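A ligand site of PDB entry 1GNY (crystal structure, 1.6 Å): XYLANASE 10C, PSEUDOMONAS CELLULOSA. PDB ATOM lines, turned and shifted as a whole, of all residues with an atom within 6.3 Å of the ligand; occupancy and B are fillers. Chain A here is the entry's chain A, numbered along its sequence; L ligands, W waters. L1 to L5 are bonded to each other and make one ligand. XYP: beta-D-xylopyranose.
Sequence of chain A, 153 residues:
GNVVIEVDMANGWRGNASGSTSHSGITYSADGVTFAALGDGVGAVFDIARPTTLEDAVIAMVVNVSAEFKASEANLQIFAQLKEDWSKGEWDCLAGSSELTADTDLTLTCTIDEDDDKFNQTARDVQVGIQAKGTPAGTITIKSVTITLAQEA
The indole nitrogen (NE1) of Trp 91 is in hydrogen-bond range of the backbone carbonyl oxygen (O) of Ser 87 (3.3 Å). OG of Ser 18 lies within hydrogen-bond range of OE1 of Gln 131 (2.7 Å). NE2 of Gln 127 lies within hydrogen-bond range of OE1 of Gln 81, at 2.8 Å. O of Trp 91 sits at hydrogen-bond distance from NE2 of Gln 77. O of Trp 86 lies within hydrogen-bond range of NE2 of Gln 81, 2.8 Å away.
An oxygen (O2) of XYP L2 is in hydrogen-bond range of the side-chain amide nitrogen (ND2) of Asn 16 (2.6 Å). An oxygen (O2) of XYP L2 lies within hydrogen-bond range of the side-chain amide nitrogen (NE2) of Gln 127 (3.0 Å). O3 of XYP L2 sits at hydrogen-bond distance from OE1 of Gln 81.
Water W7 lies within hydrogen-bond range of O2 of XYP L4, NE2 of Gln 131 and OE1 of Gln 77. Water W5 lies within hydrogen-bond range of O of Ser 87 (2.7 Å) and O5 of XYP L4 (2.9 Å). Water W4 lies within hydrogen-bond range of N of Ala 17, O4 of XYP L1 and ND2 of Asn 16. Water W8 lies within hydrogen-bond range of the side-chain hydroxyl (OG) of Ser 18, the side-chain amino group (NZ) of Lys 133 and an oxygen (O2) of XYP L4. Water W10 bridges OE2 of Glu 84 (2.5 Å) and O1 of XYP L1 (3.4 Å). Water W1 lies within hydrogen-bond range of the side-chain amide nitrogen (NE2) of Gln 77 (3.0 Å) and the backbone carbonyl oxygen (O) of Trp 91 (3.5 Å).
Merely in contact with the ligand: Trp 86, Trp 91, Ser 18, Ala 17, Ser 87 and Asp 92. Hydrophobic or aromatic side chains within 4 Å of the ligand: Trp 86 and Trp 91.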
ATOM      1  N   ASN A  16     -36.216   4.200 -14.561  1.00  0.00           N
ATOM      2  CA  ASN A  16     -35.215   3.192 -14.103  1.00  0.00           C
ATOM      3  C   ASN A  16     -35.678   2.418 -12.873  1.00  0.00           C
ATOM      4  O   ASN A  16     -36.387   2.956 -11.994  1.00  0.00           O
ATOM      5  CB  ASN A  16     -33.902   3.863 -13.744  1.00  0.00           C
ATOM      6  CG  ASN A  16     -32.727   2.917 -13.762  1.00  0.00           C
ATOM      7  OD1 ASN A  16     -32.062   2.667 -12.720  1.00  0.00           O
ATOM      8  ND2 ASN A  16     -32.412   2.434 -14.915  1.00  0.00           N
ATOM      9  N   ALA A  17     -35.315   1.134 -12.855  1.00  0.00           N
ATOM     10  CA  ALA A  17     -35.540   0.267 -11.680  1.00  0.00           C
ATOM     11  C   ALA A  17     -34.241  -0.448 -11.351  1.00  0.00           C
ATOM     12  O   ALA A  17     -33.685  -1.161 -12.164  1.00  0.00           O
ATOM     13  CB  ALA A  17     -36.616  -0.731 -11.936  1.00  0.00           C
ATOM     14  N   SER A  18     -33.732  -0.225 -10.147  1.00  0.00           N
ATOM     15  CA  SER A  18     -32.510  -0.920  -9.672  1.00  0.00           C
ATOM     16  C   SER A  18     -32.760  -1.973  -8.581  1.00  0.00           C
ATOM     17  O   SER A  18     -31.816  -2.627  -8.112  1.00  0.00           O
ATOM     18  CB  SER A  18     -31.515   0.137  -9.134  1.00  0.00           C
ATOM     19  OG  SER A  18     -32.026   0.730  -7.917  1.00  0.00           O
ATOM     20  N   GLY A  19     -34.002  -2.090  -8.147  1.00  0.00           N
ATOM     21  CA  GLY A  19     -34.450  -2.972  -7.064  1.00  0.00           C
ATOM     22  C   GLY A  19     -35.553  -3.917  -7.532  1.00  0.00           C
ATOM     23  O   GLY A  19     -35.614  -4.245  -8.705  1.00  0.00           O
ATOM     24  N   VAL A  45     -33.282   8.432 -15.003  1.00  0.00           N
ATOM     25  CA  VAL A  45     -31.886   8.471 -15.449  1.00  0.00           C
ATOM     26  C   VAL A  45     -31.685   9.060 -16.852  1.00  0.00           C
ATOM     27  O   VAL A  45     -32.645   9.123 -17.632  1.00  0.00           O
ATOM     28  CB  VAL A  45     -31.243   7.042 -15.456  1.00  0.00           C
ATOM     29  CG1 VAL A  45     -31.154   6.416 -14.040  1.00  0.00           C
ATOM     30  CG2 VAL A  45     -31.923   6.121 -16.417  1.00  0.00           C
ATOM     31  N   GLN A  77     -31.686   9.169  -3.482  1.00  0.00           N
ATOM     32  CA  GLN A  77     -30.298   8.836  -3.806  1.00  0.00           C
ATOM     33  C   GLN A  77     -29.929   9.223  -5.235  1.00  0.00           C
ATOM     34  O   GLN A  77     -30.464   8.639  -6.168  1.00  0.00           O
ATOM     35  CB  GLN A  77     -30.031   7.334  -3.624  1.00  0.00           C
ATOM     36  CG  GLN A  77     -28.607   6.907  -4.041  1.00  0.00           C
ATOM     37  CD  GLN A  77     -28.326   5.438  -3.801  1.00  0.00           C
ATOM     38  OE1 GLN A  77     -29.222   4.583  -3.808  1.00  0.00           O
ATOM     39  NE2 GLN A  77     -27.059   5.134  -3.603  1.00  0.00           N
ATOM     40  N   PHE A  79     -27.182   8.888  -7.999  1.00  0.00           N
ATOM     41  CA  PHE A  79     -26.189   7.840  -8.256  1.00  0.00           C
ATOM     42  C   PHE A  79     -25.645   7.929  -9.678  1.00  0.00           C
ATOM     43  O   PHE A  79     -26.223   8.592 -10.510  1.00  0.00           O
ATOM     44  CB  PHE A  79     -26.802   6.445  -8.004  1.00  0.00           C
ATOM     45  CG  PHE A  79     -27.926   6.079  -8.940  1.00  0.00           C
ATOM     46  CD1 PHE A  79     -29.210   6.589  -8.771  1.00  0.00           C
ATOM     47  CD2 PHE A  79     -27.692   5.232 -10.014  1.00  0.00           C
ATOM     48  CE1 PHE A  79     -30.251   6.260  -9.638  1.00  0.00           C
ATOM     49  CE2 PHE A  79     -28.696   4.931 -10.901  1.00  0.00           C
ATOM     50  CZ  PHE A  79     -30.000   5.429 -10.706  1.00  0.00           C
ATOM     51  N   GLN A  81     -23.383   5.133 -12.587  1.00  0.00           N
ATOM     52  CA  GLN A  81     -22.826   3.775 -12.790  1.00  0.00           C
ATOM     53  C   GLN A  81     -22.444   3.599 -14.267  1.00  0.00           C
ATOM     54  O   GLN A  81     -22.963   4.261 -15.168  1.00  0.00           O
ATOM     55  CB  GLN A  81     -23.840   2.668 -12.366  1.00  0.00           C
ATOM     56  CG  GLN A  81     -25.167   2.756 -13.136  1.00  0.00           C
ATOM     57  CD  GLN A  81     -26.346   1.916 -12.576  1.00  0.00           C
ATOM     58  OE1 GLN A  81     -27.496   2.330 -12.755  1.00  0.00           O
ATOM     59  NE2 GLN A  81     -26.069   0.718 -12.026  1.00  0.00           N
ATOM     60  N   GLU A  84     -23.998  -0.929 -18.751  1.00  0.00           N
ATOM     61  CA  GLU A  84     -23.691  -2.310 -19.070  1.00  0.00           C
ATOM     62  C   GLU A  84     -22.627  -2.982 -18.167  1.00  0.00           C
ATOM     63  O   GLU A  84     -22.232  -4.106 -18.430  1.00  0.00           O
ATOM     64  CB  GLU A  84     -23.314  -2.444 -20.546  1.00  0.00           C
ATOM     65  CG  GLU A  84     -24.150  -3.451 -21.275  1.00  0.00           C
ATOM     66  CD  GLU A  84     -25.593  -3.002 -21.362  1.00  0.00           C
ATOM     67  OE1 GLU A  84     -25.873  -2.005 -22.064  1.00  0.00           O
ATOM     68  OE2 GLU A  84     -26.433  -3.632 -20.681  1.00  0.00           O
ATOM     69  N   TRP A  86     -23.091  -2.574 -14.591  1.00  0.00           N
ATOM     70  CA  TRP A  86     -23.955  -1.905 -13.587  1.00  0.00           C
ATOM     71  C   TRP A  86     -23.524  -1.804 -12.130  1.00  0.00           C
ATOM     72  O   TRP A  86     -23.836  -0.825 -11.483  1.00  0.00           O
ATOM     73  CB  TRP A  86     -25.360  -2.503 -13.652  1.00  0.00           C
ATOM     74  CG  TRP A  86     -25.953  -2.622 -15.031  1.00  0.00           C
ATOM     75  CD1 TRP A  86     -26.187  -3.771 -15.720  1.00  0.00           C
ATOM     76  CD2 TRP A  86     -26.425  -1.558 -15.877  1.00  0.00           C
ATOM     77  NE1 TRP A  86     -26.812  -3.502 -16.908  1.00  0.00           N
ATOM     78  CE2 TRP A  86     -26.947  -2.147 -17.043  1.00  0.00           C
ATOM     79  CE3 TRP A  86     -26.456  -0.167 -15.751  1.00  0.00           C
ATOM     80  CZ2 TRP A  86     -27.488  -1.403 -18.094  1.00  0.00           C
ATOM     81  CZ3 TRP A  86     -26.998   0.574 -16.771  1.00  0.00           C
ATOM     82  CH2 TRP A  86     -27.499  -0.039 -17.942  1.00  0.00           C
ATOM     83  N   SER A  87     -22.795  -2.797 -11.617  1.00  0.00           N
ATOM     84  CA  SER A  87     -22.362  -2.799 -10.191  1.00  0.00           C
ATOM     85  C   SER A  87     -21.258  -1.765  -9.860  1.00  0.00           C
ATOM     86  O   SER A  87     -21.088  -1.403  -8.687  1.00  0.00           O
ATOM     87  CB  SER A  87     -21.852  -4.162  -9.778  1.00  0.00           C
ATOM     88  OG  SER A  87     -20.548  -4.306 -10.268  1.00  0.00           O
ATOM     89  N   LYS A  88     -20.554  -1.338 -10.885  1.00  0.00           N
ATOM     90  CA  LYS A  88     -19.490  -0.375 -10.760  1.00  0.00           C
ATOM     91  C   LYS A  88     -20.100   1.029 -10.792  1.00  0.00           C
ATOM     92  O   LYS A  88     -20.555   1.493 -11.843  1.00  0.00           O
ATOM     93  CB  LYS A  88     -18.498  -0.567 -11.899  1.00  0.00           C
ATOM     94  CG  LYS A  88     -17.960  -2.009 -12.096  1.00  0.00           C
ATOM     95  CD  LYS A  88     -17.333  -2.568 -10.821  1.00  0.00           C
ATOM     96  CE  LYS A  88     -16.909  -4.049 -10.964  1.00  0.00           C
ATOM     97  NZ  LYS A  88     -15.968  -4.243 -12.089  1.00  0.00           N
ATOM     98  N   TRP A  91     -22.262   5.016  -5.130  1.00  0.00           N
ATOM     99  CA  TRP A  91     -23.404   4.618  -4.294  1.00  0.00           C
ATOM    100  C   TRP A  91     -23.434   5.300  -2.912  1.00  0.00           C
ATOM    101  O   TRP A  91     -24.259   4.951  -2.073  1.00  0.00           O
ATOM    102  CB  TRP A  91     -23.289   3.087  -4.100  1.00  0.00           C
ATOM    103  CG  TRP A  91     -23.207   2.354  -5.413  1.00  0.00           C
ATOM    104  CD1 TRP A  91     -22.147   1.651  -5.942  1.00  0.00           C
ATOM    105  CD2 TRP A  91     -24.252   2.260  -6.375  1.00  0.00           C
ATOM    106  NE1 TRP A  91     -22.484   1.142  -7.171  1.00  0.00           N
ATOM    107  CE2 TRP A  91     -23.767   1.503  -7.458  1.00  0.00           C
ATOM    108  CE3 TRP A  91     -25.578   2.730  -6.412  1.00  0.00           C
ATOM    109  CZ2 TRP A  91     -24.557   1.203  -8.583  1.00  0.00           C
ATOM    110  CZ3 TRP A  91     -26.363   2.430  -7.517  1.00  0.00           C
ATOM    111  CH2 TRP A  91     -25.836   1.688  -8.592  1.00  0.00           C
ATOM    112  N   ASP A  92     -22.577   6.267  -2.677  1.00  0.00           N
ATOM    113  CA  ASP A  92     -22.443   6.866  -1.320  1.00  0.00           C
ATOM    114  C   ASP A  92     -23.187   8.198  -1.064  1.00  0.00           C
ATOM    115  O   ASP A  92     -23.045   8.805   0.021  1.00  0.00           O
ATOM    116  CB  ASP A  92     -20.945   7.027  -0.954  1.00  0.00           C
ATOM    117  CG  ASP A  92     -20.198   5.686  -0.899  1.00  0.00           C
ATOM    118  OD1 ASP A  92     -20.785   4.619  -0.575  1.00  0.00           O
ATOM    119  OD2 ASP A  92     -18.982   5.608  -1.209  1.00  0.00           O
ATOM    120  N   GLN A 127     -24.427   6.096 -16.866  1.00  0.00           N
ATOM    121  CA  GLN A 127     -25.826   6.324 -16.506  1.00  0.00           C
ATOM    122  C   GLN A 127     -25.892   7.064 -15.198  1.00  0.00           C
ATOM    123  O   GLN A 127     -25.303   6.584 -14.215  1.00  0.00           O
ATOM    124  CB  GLN A 127     -26.603   5.030 -16.396  1.00  0.00           C
ATOM    125  CG  GLN A 127     -28.094   5.159 -16.071  1.00  0.00           C
ATOM    126  CD  GLN A 127     -28.800   3.818 -16.178  1.00  0.00           C
ATOM    127  OE1 GLN A 127     -29.324   3.501 -17.263  1.00  0.00           O
ATOM    128  NE2 GLN A 127     -28.862   3.076 -15.071  1.00  0.00           N
ATOM    129  N   GLN A 131     -33.046   8.197  -7.513  1.00  0.00           N
ATOM    130  CA  GLN A 131     -34.011   7.133  -7.207  1.00  0.00           C
ATOM    131  C   GLN A 131     -34.515   7.208  -5.757  1.00  0.00           C
ATOM    132  O   GLN A 131     -33.796   7.743  -4.885  1.00  0.00           O
ATOM    133  CB  GLN A 131     -33.410   5.734  -7.474  1.00  0.00           C
ATOM    134  CG  GLN A 131     -32.175   5.404  -6.602  1.00  0.00           C
ATOM    135  CD  GLN A 131     -31.562   4.029  -6.945  1.00  0.00           C
ATOM    136  OE1 GLN A 131     -32.019   3.380  -7.899  1.00  0.00           O
ATOM    137  NE2 GLN A 131     -30.550   3.595  -6.144  1.00  0.00           N
ATOM    138  N   LYS A 133     -35.565   5.534  -2.189  1.00  0.00           N
ATOM    139  CA  LYS A 133     -35.122   4.414  -1.334  1.00  0.00           C
ATOM    140  C   LYS A 133     -36.027   4.340  -0.091  1.00  0.00           C
ATOM    141  O   LYS A 133     -36.244   5.344   0.571  1.00  0.00           O
ATOM    142  CB  LYS A 133     -33.679   4.574  -0.849  1.00  0.00           C
ATOM    143  CG  LYS A 133     -32.591   4.727  -1.926  1.00  0.00           C
ATOM    144  CD  LYS A 133     -32.378   3.482  -2.687  1.00  0.00           C
ATOM    145  CE  LYS A 133     -31.482   2.439  -1.982  1.00  0.00           C
ATOM    146  NZ  LYS A 133     -31.847   1.094  -2.631  1.00  0.00           N
HETATM  147  O1  XYP L   1     -31.945  -4.149 -20.629  1.00  0.00           O
HETATM  148  C1  XYP L   1     -32.226  -3.359 -19.489  1.00  0.00           C
HETATM  149  C2  XYP L   1     -32.819  -4.232 -18.428  1.00  0.00           C
HETATM  150  C3  XYP L   1     -32.951  -3.487 -17.112  1.00  0.00           C
HETATM  151  C4  XYP L   1     -31.647  -2.771 -16.792  1.00  0.00           C
HETATM  152  C5  XYP L   1     -31.278  -1.910 -17.987  1.00  0.00           C
HETATM  153  O2  XYP L   1     -34.101  -4.488 -18.926  1.00  0.00           O
HETATM  154  O3  XYP L   1     -33.232  -4.344 -16.035  1.00  0.00           O
HETATM  155  O4  XYP L   1     -31.850  -1.960 -15.664  1.00  0.00           O
HETATM  156  O5  XYP L   1     -31.052  -2.828 -19.037  1.00  0.00           O
HETATM  157  C1  XYP L   2     -30.624  -1.823 -14.951  1.00  0.00           C
HETATM  158  C2  XYP L   2     -30.682  -0.466 -14.266  1.00  0.00           C
HETATM  159  C3  XYP L   2     -29.515  -0.304 -13.287  1.00  0.00           C
HETATM  160  C4  XYP L   2     -29.381  -1.550 -12.406  1.00  0.00           C
HETATM  161  C5  XYP L   2     -29.378  -2.780 -13.285  1.00  0.00           C
HETATM  162  O2  XYP L   2     -30.593   0.574 -15.228  1.00  0.00           O
HETATM  163  O3  XYP L   2     -29.698   0.851 -12.481  1.00  0.00           O
HETATM  164  O4  XYP L   2     -28.146  -1.451 -11.716  1.00  0.00           O
HETATM  165  O5  XYP L   2     -30.538  -2.860 -14.079  1.00  0.00           O
HETATM  166  C1  XYP L   3     -28.102  -1.873 -10.352  1.00  0.00           C
HETATM  167  C2  XYP L   3     -26.850  -2.710 -10.175  1.00  0.00           C
HETATM  168  C3  XYP L   3     -26.762  -3.123  -8.719  1.00  0.00           C
HETATM  169  C4  XYP L   3     -26.798  -1.909  -7.820  1.00  0.00           C
HETATM  170  C5  XYP L   3     -28.022  -1.097  -8.171  1.00  0.00           C
HETATM  171  O2  XYP L   3     -26.910  -3.875 -10.985  1.00  0.00           O
HETATM  172  O3  XYP L   3     -25.527  -3.750  -8.446  1.00  0.00           O
HETATM  173  O4  XYP L   3     -26.878  -2.336  -6.462  1.00  0.00           O
HETATM  174  O5  XYP L   3     -28.057  -0.775  -9.578  1.00  0.00           O
HETATM  175  C1  XYP L   4     -26.238  -1.468  -5.562  1.00  0.00           C
HETATM  176  C2  XYP L   4     -26.938  -1.612  -4.220  1.00  0.00           C
HETATM  177  C3  XYP L   4     -26.202  -0.852  -3.148  1.00  0.00           C
HETATM  178  C4  XYP L   4     -24.723  -1.187  -3.197  1.00  0.00           C
HETATM  179  C5  XYP L   4     -24.239  -0.982  -4.614  1.00  0.00           C
HETATM  180  O2  XYP L   4     -28.274  -1.152  -4.307  1.00  0.00           O
HETATM  181  O3  XYP L   4     -26.722  -1.135  -1.856  1.00  0.00           O
HETATM  182  O4  XYP L   4     -24.109  -0.273  -2.322  1.00  0.00           O
HETATM  183  O5  XYP L   4     -24.948  -1.823  -5.516  1.00  0.00           O
HETATM  184  C1  XYP L   5     -22.983  -0.806  -1.583  1.00  0.00           C
HETATM  185  C2  XYP L   5     -22.136   0.316  -0.994  1.00  0.00           C
HETATM  186  C3  XYP L   5     -21.162  -0.141   0.109  1.00  0.00           C
HETATM  187  C4  XYP L   5     -21.630  -1.358   0.900  1.00  0.00           C
HETATM  188  C5  XYP L   5     -22.418  -2.332   0.032  1.00  0.00           C
HETATM  189  O2  XYP L   5     -21.324   0.994  -1.937  1.00  0.00           O
HETATM  190  O3  XYP L   5     -20.935   0.930   1.008  1.00  0.00           O
HETATM  191  O4  XYP L   5     -20.489  -1.993   1.417  1.00  0.00           O
HETATM  192  O5  XYP L   5     -23.453  -1.632  -0.609  1.00  0.00           O
HETATM  193  O   HOH W   1     -26.714   2.488  -2.266  1.00  0.00           O
HETATM  194  O   HOH W   2     -25.979  -3.067  -0.223  1.00  0.00           O
HETATM  195  O   HOH W   3     -32.932  -3.964 -13.246  1.00  0.00           O
HETATM  196  O   HOH W   4     -34.375  -0.219 -15.358  1.00  0.00           O
HETATM  197  O   HOH W   5     -22.466  -2.657  -6.735  1.00  0.00           O
HETATM  198  O   HOH W   6     -21.113  -1.627   3.906  1.00  0.00           O
HETATM  199  O   HOH W   7     -29.186   1.402  -4.933  1.00  0.00           O
HETATM  200  O   HOH W   8     -31.232  -0.174  -5.553  1.00  0.00           O
HETATM  201  O   HOH W   9     -24.557  -5.753 -10.170  1.00  0.00           O
HETATM  202  O   HOH W  10     -28.700  -4.293 -21.489  1.00  0.00           O
